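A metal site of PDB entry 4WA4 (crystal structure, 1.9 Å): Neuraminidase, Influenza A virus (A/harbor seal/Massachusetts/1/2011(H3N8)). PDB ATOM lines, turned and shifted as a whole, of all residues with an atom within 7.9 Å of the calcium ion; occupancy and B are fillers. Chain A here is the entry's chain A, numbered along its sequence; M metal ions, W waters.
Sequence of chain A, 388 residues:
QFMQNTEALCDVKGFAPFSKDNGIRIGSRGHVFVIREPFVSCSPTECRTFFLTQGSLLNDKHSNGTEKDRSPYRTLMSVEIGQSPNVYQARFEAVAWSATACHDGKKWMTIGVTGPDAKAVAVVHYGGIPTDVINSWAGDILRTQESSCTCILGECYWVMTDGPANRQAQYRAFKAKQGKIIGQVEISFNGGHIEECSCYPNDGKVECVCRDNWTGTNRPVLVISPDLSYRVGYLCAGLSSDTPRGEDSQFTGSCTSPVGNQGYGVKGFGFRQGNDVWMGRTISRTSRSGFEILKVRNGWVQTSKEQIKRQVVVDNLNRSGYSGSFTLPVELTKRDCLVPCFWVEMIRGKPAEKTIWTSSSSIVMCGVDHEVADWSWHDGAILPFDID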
ATOM      1  N   HIS A 193      18.204  -7.705 -29.246  1.00  0.00           N
ATOM      2  CA  HIS A 193      18.497  -8.013 -27.899  1.00  0.00           C
ATOM      3  C   HIS A 193      17.992  -6.893 -27.043  1.00  0.00           C
ATOM      4  O   HIS A 193      18.082  -5.678 -27.433  1.00  0.00           O
ATOM      5  CB  HIS A 193      19.992  -8.138 -27.769  1.00  0.00           C
ATOM      6  CG  HIS A 193      20.419  -8.798 -26.514  1.00  0.00           C
ATOM      7  ND1 HIS A 193      20.892  -8.094 -25.409  1.00  0.00           N
ATOM      8  CD2 HIS A 193      20.375 -10.099 -26.157  1.00  0.00           C
ATOM      9  CE1 HIS A 193      21.182  -8.951 -24.459  1.00  0.00           C
ATOM     10  NE2 HIS A 193      20.894 -10.189 -24.897  1.00  0.00           N
ATOM     11  N   ARG A 211      18.295  -1.643 -23.869  1.00  0.00           N
ATOM     12  CA  ARG A 211      19.678  -1.855 -24.040  1.00  0.00           C
ATOM     13  C   ARG A 211      19.861  -3.125 -24.865  1.00  0.00           C
ATOM     14  O   ARG A 211      19.371  -4.246 -24.453  1.00  0.00           O
ATOM     15  CB  ARG A 211      20.322  -1.941 -22.669  1.00  0.00           C
ATOM     16  CG  ARG A 211      21.730  -2.562 -22.642  1.00  0.00           C
ATOM     17  CD  ARG A 211      22.248  -2.714 -21.242  1.00  0.00           C
ATOM     18  NE  ARG A 211      23.513  -3.436 -21.163  1.00  0.00           N
ATOM     19  CZ  ARG A 211      24.246  -3.548 -20.094  1.00  0.00           C
ATOM     20  NH1 ARG A 211      23.840  -3.043 -18.955  1.00  0.00           N
ATOM     21  NH2 ARG A 211      25.407  -4.161 -20.110  1.00  0.00           N
ATOM     22  N   ASP A 212      20.589  -3.026 -25.997  1.00  0.00           N
ATOM     23  CA  ASP A 212      21.025  -4.151 -26.815  1.00  0.00           C
ATOM     24  C   ASP A 212      22.430  -4.498 -26.384  1.00  0.00           C
ATOM     25  O   ASP A 212      23.327  -3.709 -26.491  1.00  0.00           O
ATOM     26  CB  ASP A 212      20.891  -3.873 -28.334  1.00  0.00           C
ATOM     27  CG  ASP A 212      21.454  -4.985 -29.230  1.00  0.00           C
ATOM     28  OD1 ASP A 212      22.487  -5.604 -28.855  1.00  0.00           O
ATOM     29  OD2 ASP A 212      20.884  -5.198 -30.358  1.00  0.00           O
ATOM     30  N   ASN A 213      22.643  -5.693 -25.774  1.00  0.00           N
ATOM     31  CA  ASN A 213      23.934  -6.038 -25.209  1.00  0.00           C
ATOM     32  C   ASN A 213      24.693  -7.024 -26.143  1.00  0.00           C
ATOM     33  O   ASN A 213      25.719  -7.557 -25.782  1.00  0.00           O
ATOM     34  CB  ASN A 213      23.765  -6.618 -23.824  1.00  0.00           C
ATOM     35  CG  ASN A 213      24.935  -6.343 -22.923  1.00  0.00           C
ATOM     36  OD1 ASN A 213      25.327  -5.183 -22.731  1.00  0.00           O
ATOM     37  ND2 ASN A 213      25.519  -7.352 -22.372  1.00  0.00           N
ATOM     38  N   TRP A 214      24.136  -7.257 -27.301  1.00  0.00           N
ATOM     39  CA  TRP A 214      24.675  -8.252 -28.268  1.00  0.00           C
ATOM     40  C   TRP A 214      25.466  -7.602 -29.356  1.00  0.00           C
ATOM     41  O   TRP A 214      26.701  -7.648 -29.317  1.00  0.00           O
ATOM     42  CB  TRP A 214      23.472  -9.054 -28.826  1.00  0.00           C
ATOM     43  CG  TRP A 214      23.794 -10.134 -29.786  1.00  0.00           C
ATOM     44  CD1 TRP A 214      24.995 -10.642 -30.071  1.00  0.00           C
ATOM     45  CD2 TRP A 214      22.823 -10.875 -30.522  1.00  0.00           C
ATOM     46  NE1 TRP A 214      24.871 -11.685 -31.025  1.00  0.00           N
ATOM     47  CE2 TRP A 214      23.539 -11.838 -31.304  1.00  0.00           C
ATOM     48  CE3 TRP A 214      21.397 -10.832 -30.585  1.00  0.00           C
ATOM     49  CZ2 TRP A 214      22.883 -12.746 -32.154  1.00  0.00           C
ATOM     50  CZ3 TRP A 214      20.735 -11.739 -31.458  1.00  0.00           C
ATOM     51  CH2 TRP A 214      21.514 -12.715 -32.198  1.00  0.00           C
ATOM     52  N   THR A 215      24.824  -6.994 -30.345  1.00  0.00           N
ATOM     53  CA  THR A 215      25.524  -6.307 -31.412  1.00  0.00           C
ATOM     54  C   THR A 215      25.193  -4.809 -31.642  1.00  0.00           C
ATOM     55  O   THR A 215      25.907  -4.119 -32.370  1.00  0.00           O
ATOM     56  CB  THR A 215      25.294  -6.953 -32.819  1.00  0.00           C
ATOM     57  OG1 THR A 215      23.923  -6.741 -33.253  1.00  0.00           O
ATOM     58  CG2 THR A 215      25.548  -8.491 -32.766  1.00  0.00           C
ATOM     59  N   GLY A 216      24.147  -4.298 -31.007  1.00  0.00           N
ATOM     60  CA  GLY A 216      23.657  -2.954 -31.319  1.00  0.00           C
ATOM     61  C   GLY A 216      24.292  -1.800 -30.463  1.00  0.00           C
ATOM     62  O   GLY A 216      24.487  -1.917 -29.237  1.00  0.00           O
ATOM     63  N   THR A 217      24.575  -0.683 -31.156  1.00  0.00           N
ATOM     64  CA  THR A 217      25.039   0.564 -30.488  1.00  0.00           C
ATOM     65  C   THR A 217      23.931   1.562 -30.435  1.00  0.00           C
ATOM     66  O   THR A 217      24.049   2.577 -29.772  1.00  0.00           O
ATOM     67  CB  THR A 217      26.289   1.236 -31.133  1.00  0.00           C
ATOM     68  OG1 THR A 217      25.953   1.580 -32.438  1.00  0.00           O
ATOM     69  CG2 THR A 217      27.521   0.341 -31.174  1.00  0.00           C
ATOM     70  N   ASN A 218      22.863   1.242 -31.127  1.00  0.00           N
ATOM     71  CA  ASN A 218      21.641   1.900 -31.022  1.00  0.00           C
ATOM     72  C   ASN A 218      20.696   1.187 -30.038  1.00  0.00           C
ATOM     73  O   ASN A 218      20.903   0.003 -29.688  1.00  0.00           O
ATOM     74  CB  ASN A 218      21.010   2.088 -32.395  1.00  0.00           C
ATOM     75  CG  ASN A 218      20.827   0.777 -33.202  1.00  0.00           C
ATOM     76  OD1 ASN A 218      21.527  -0.184 -32.989  1.00  0.00           O
ATOM     77  ND2 ASN A 218      19.907   0.812 -34.194  1.00  0.00           N
ATOM     78  N   ARG A 219      19.634   1.867 -29.597  1.00  0.00           N
ATOM     79  CA  ARG A 219      18.756   1.230 -28.592  1.00  0.00           C
ATOM     80  C   ARG A 219      17.471   0.686 -29.140  1.00  0.00           C
ATOM     81  O   ARG A 219      16.823   1.318 -29.958  1.00  0.00           O
ATOM     82  CB  ARG A 219      18.447   2.203 -27.490  1.00  0.00           C
ATOM     83  CG  ARG A 219      19.661   2.595 -26.645  1.00  0.00           C
ATOM     84  CD  ARG A 219      19.201   3.454 -25.465  1.00  0.00           C
ATOM     85  NE  ARG A 219      20.340   3.775 -24.652  1.00  0.00           N
ATOM     86  CZ  ARG A 219      20.974   2.960 -23.828  1.00  0.00           C
ATOM     87  NH1 ARG A 219      22.078   3.368 -23.220  1.00  0.00           N
ATOM     88  NH2 ARG A 219      20.603   1.714 -23.727  1.00  0.00           N
ATOM     89  N   PRO A 220      17.052  -0.508 -28.657  1.00  0.00           N
ATOM     90  CA  PRO A 220      15.737  -1.010 -28.939  1.00  0.00           C
ATOM     91  C   PRO A 220      14.604  -0.174 -28.446  1.00  0.00           C
ATOM     92  O   PRO A 220      14.677   0.487 -27.424  1.00  0.00           O
ATOM     93  CB  PRO A 220      15.736  -2.427 -28.321  1.00  0.00           C
ATOM     94  CG  PRO A 220      17.128  -2.746 -28.029  1.00  0.00           C
ATOM     95  CD  PRO A 220      17.884  -1.464 -27.905  1.00  0.00           C
ATOM     96  N   ASP A 242      24.020   4.128 -27.009  1.00  0.00           N
ATOM     97  CA  ASP A 242      24.572   3.142 -26.132  1.00  0.00           C
ATOM     98  C   ASP A 242      25.987   3.454 -25.798  1.00  0.00           C
ATOM     99  O   ASP A 242      26.581   4.387 -26.420  1.00  0.00           O
ATOM    100  CB  ASP A 242      24.459   1.719 -26.773  1.00  0.00           C
ATOM    101  CG  ASP A 242      24.391   0.584 -25.671  1.00  0.00           C
ATOM    102  OD1 ASP A 242      24.348   0.920 -24.452  1.00  0.00           O
ATOM    103  OD2 ASP A 242      24.336  -0.614 -26.010  1.00  0.00           O
ATOM    104  N   THR A 243      26.558   2.720 -24.844  1.00  0.00           N
ATOM    105  CA  THR A 243      27.962   2.721 -24.626  1.00  0.00           C
ATOM    106  C   THR A 243      28.420   1.335 -24.274  1.00  0.00           C
ATOM    107  O   THR A 243      27.865   0.675 -23.378  1.00  0.00           O
ATOM    108  CB  THR A 243      28.509   3.872 -23.735  1.00  0.00           C
ATOM    109  OG1 THR A 243      29.255   3.402 -22.651  1.00  0.00           O
ATOM    110  CG2 THR A 243      27.505   4.802 -23.324  1.00  0.00           C
ATOM    111  N   PRO A 244      29.435   0.822 -25.032  1.00  0.00           N
ATOM    112  CA  PRO A 244      30.213   1.490 -26.090  1.00  0.00           C
ATOM    113  C   PRO A 244      29.516   1.716 -27.402  1.00  0.00           C
ATOM    114  O   PRO A 244      28.516   1.090 -27.707  1.00  0.00           O
ATOM    115  CB  PRO A 244      31.419   0.552 -26.307  1.00  0.00           C
ATOM    116  CG  PRO A 244      30.957  -0.772 -25.855  1.00  0.00           C
ATOM    117  CD  PRO A 244      29.991  -0.490 -24.722  1.00  0.00           C
ATOM    118  N   ARG A 245      29.981   2.730 -28.105  1.00  0.00           N
ATOM    119  CA  ARG A 245      29.475   3.040 -29.398  1.00  0.00           C
ATOM    120  C   ARG A 245      30.613   3.654 -30.272  1.00  0.00           C
ATOM    121  O   ARG A 245      31.684   4.046 -29.783  1.00  0.00           O
ATOM    122  CB  ARG A 245      28.291   4.018 -29.281  1.00  0.00           C
ATOM    123  CG  ARG A 245      28.713   5.423 -28.782  1.00  0.00           C
ATOM    124  CD  ARG A 245      27.591   6.421 -28.709  1.00  0.00           C
ATOM    125  NE  ARG A 245      28.043   7.714 -28.170  1.00  0.00           N
ATOM    126  CZ  ARG A 245      28.078   8.035 -26.883  1.00  0.00           C
ATOM    127  NH1 ARG A 245      27.602   7.152 -25.956  1.00  0.00           N
ATOM    128  NH2 ARG A 245      28.570   9.223 -26.537  1.00  0.00           N
ATOM    129  N   VAL A 259      22.672  -1.556 -35.269  1.00  0.00           N
ATOM    130  CA  VAL A 259      23.787  -1.006 -35.997  1.00  0.00           C
ATOM    131  C   VAL A 259      25.000  -0.790 -35.094  1.00  0.00           C
ATOM    132  O   VAL A 259      24.850  -0.525 -33.903  1.00  0.00           O
ATOM    133  CB  VAL A 259      23.367   0.323 -36.610  1.00  0.00           C
ATOM    134  CG1 VAL A 259      24.602   0.918 -37.345  1.00  0.00           C
ATOM    135  CG2 VAL A 259      22.197   0.148 -37.551  1.00  0.00           C
ATOM    136  N   ASN A 261      27.900  -2.978 -34.793  1.00  0.00           N
ATOM    137  CA  ASN A 261      28.660  -4.224 -34.494  1.00  0.00           C
ATOM    138  C   ASN A 261      29.638  -4.149 -33.282  1.00  0.00           C
ATOM    139  O   ASN A 261      30.823  -4.292 -33.442  1.00  0.00           O
ATOM    140  CB  ASN A 261      29.431  -4.664 -35.742  1.00  0.00           C
ATOM    141  CG  ASN A 261      28.548  -4.814 -36.969  1.00  0.00           C
ATOM    142  OD1 ASN A 261      28.748  -4.134 -37.986  1.00  0.00           O
ATOM    143  ND2 ASN A 261      27.595  -5.711 -36.908  1.00  0.00           N
ATOM    144  N   GLN A 262      29.110  -3.874 -32.083  1.00  0.00           N
ATOM    145  CA  GLN A 262      29.901  -3.825 -30.872  1.00  0.00           C
ATOM    146  C   GLN A 262      29.043  -4.487 -29.818  1.00  0.00           C
ATOM    147  O   GLN A 262      27.809  -4.406 -29.839  1.00  0.00           O
ATOM    148  CB  GLN A 262      30.204  -2.409 -30.385  1.00  0.00           C
ATOM    149  CG  GLN A 262      31.204  -1.660 -31.246  1.00  0.00           C
ATOM    150  CD  GLN A 262      31.685  -0.378 -30.647  1.00  0.00           C
ATOM    151  OE1 GLN A 262      31.571   0.683 -31.222  1.00  0.00           O
ATOM    152  NE2 GLN A 262      32.285  -0.484 -29.515  1.00  0.00           N
ATOM    153  N   GLY A 263      29.725  -5.134 -28.909  1.00  0.00           N
ATOM    154  CA  GLY A 263      29.098  -5.752 -27.743  1.00  0.00           C
ATOM    155  C   GLY A 263      28.900  -4.790 -26.586  1.00  0.00           C
ATOM    156  O   GLY A 263      29.163  -3.563 -26.665  1.00  0.00           O
ATOM    157  N   TYR A 264      28.406  -5.368 -25.506  1.00  0.00           N
ATOM    158  CA  TYR A 264      28.244  -4.711 -24.244  1.00  0.00           C
ATOM    159  C   TYR A 264      27.222  -3.607 -24.380  1.00  0.00           C
ATOM    160  O   TYR A 264      26.483  -3.560 -25.346  1.00  0.00           O
ATOM    161  CB  TYR A 264      29.572  -4.160 -23.647  1.00  0.00           C
ATOM    162  CG  TYR A 264      29.488  -3.984 -22.072  1.00  0.00           C
ATOM    163  CD1 TYR A 264      28.957  -5.020 -21.236  1.00  0.00           C
ATOM    164  CD2 TYR A 264      29.940  -2.776 -21.415  1.00  0.00           C
ATOM    165  CE1 TYR A 264      28.925  -4.897 -19.825  1.00  0.00           C
ATOM    166  CE2 TYR A 264      29.871  -2.660 -20.029  1.00  0.00           C
ATOM    167  CZ  TYR A 264      29.392  -3.742 -19.239  1.00  0.00           C
ATOM    168  OH  TYR A 264      29.328  -3.664 -17.847  1.00  0.00           O
ATOM    169  N   GLY A 265      27.117  -2.716 -23.397  1.00  0.00           N
ATOM    170  CA  GLY A 265      26.043  -1.721 -23.429  1.00  0.00           C
ATOM    171  C   GLY A 265      25.904  -1.139 -22.004  1.00  0.00           C
ATOM    172  O   GLY A 265      26.694  -1.388 -21.129  1.00  0.00           O
ATOM    173  N   VAL A 266      24.925  -0.277 -21.852  1.00  0.00           N
ATOM    174  CA  VAL A 266      24.598   0.391 -20.577  1.00  0.00           C
ATOM    175  C   VAL A 266      23.108   0.658 -20.632  1.00  0.00           C
ATOM    176  O   VAL A 266      22.553   0.942 -21.720  1.00  0.00           O
ATOM    177  CB  VAL A 266      25.452   1.680 -20.300  1.00  0.00           C
ATOM    178  CG1 VAL A 266      25.128   2.799 -21.273  1.00  0.00           C
ATOM    179  CG2 VAL A 266      25.225   2.165 -18.853  1.00  0.00           C
HETATM  180 CA    CA M   1      25.275  -2.454 -27.075  1.00  0.00          CA
HETATM  181  O   HOH W   1      27.337  -1.412 -27.408  1.00  0.00           O
HETATM  182  O   HOH W   2      26.031  -4.615 -28.094  1.00  0.00           O
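Water W2 lies within hydrogen-bond range of the backbone carbonyl oxygen (O) of Gln 262 (2.5 Å), the backbone carbonyl oxygen (O) of Trp 214 (3.3 Å), the backbone NH (N) of Gly 216 (3.5 Å) and the backbone NH (N) of Thr 215 (3.5 Å).
Water W1 lies within hydrogen-bond range of the backbone carbonyl oxygen (O) of Pro 244 (2.8 Å) and the backbone carbonyl oxygen (O) of Gly 263 (2.9 Å).
The side-chain carboxylate (OD1) of Asp 242 lies within salt-bridge range of the guanidinium group (NH1) of Arg 219, 3.6 Å away.
The side-chain carboxylate (OD1) of Asp 212 is in hydrogen-bond range of the backbone NH (N) of Thr 215, 3.1 Å away.
The backbone NH (N) of Gly 265 lies within hydrogen-bond range of the side-chain amide oxygen (OD1) of Asn 213 (3.1 Å).
N of Val 266 lies within hydrogen-bond range of OD1 of Asp 242, 2.9 Å away.
The backbone NH (N) of Tyr 264 sits at hydrogen-bond distance from the backbone carbonyl oxygen (O) of Asn 213 (3.5 Å).
The backbone carbonyl oxygen (O) of Thr 217 lies close to the backbone NH (N) of Asp 242, 3.2 Å away.
The backbone NH of Gly 216 lies within hydrogen-bond range of the side-chain carboxylate of Asp 212, at 3.0 Å.
The backbone carbonyl oxygen (O) of Asp 242 lies within hydrogen-bond range of the guanidinium group (NH1) of Arg 245, at 3.0 Å.
The calcium ion is bound by OD2 of Asp 242, at 2.3 Å.
Water W1 binds the calcium ion (2.3 Å).
O of Gly 216 binds the calcium ion (2.4 Å).
O of Tyr 264 is bound to the calcium ion (2.4 Å).
The calcium ion is bound by O of Asp 212, at 2.4 Å.
Water W2 binds the calcium ion (2.5 Å).
Merely in contact with the calcium ion: Gly 265.
Of the 22 residues printed, 5 come within 4 Å of the calcium ion.
The nearest printed residue that does not touch the calcium ion is Gly 263 (4.1 Å).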
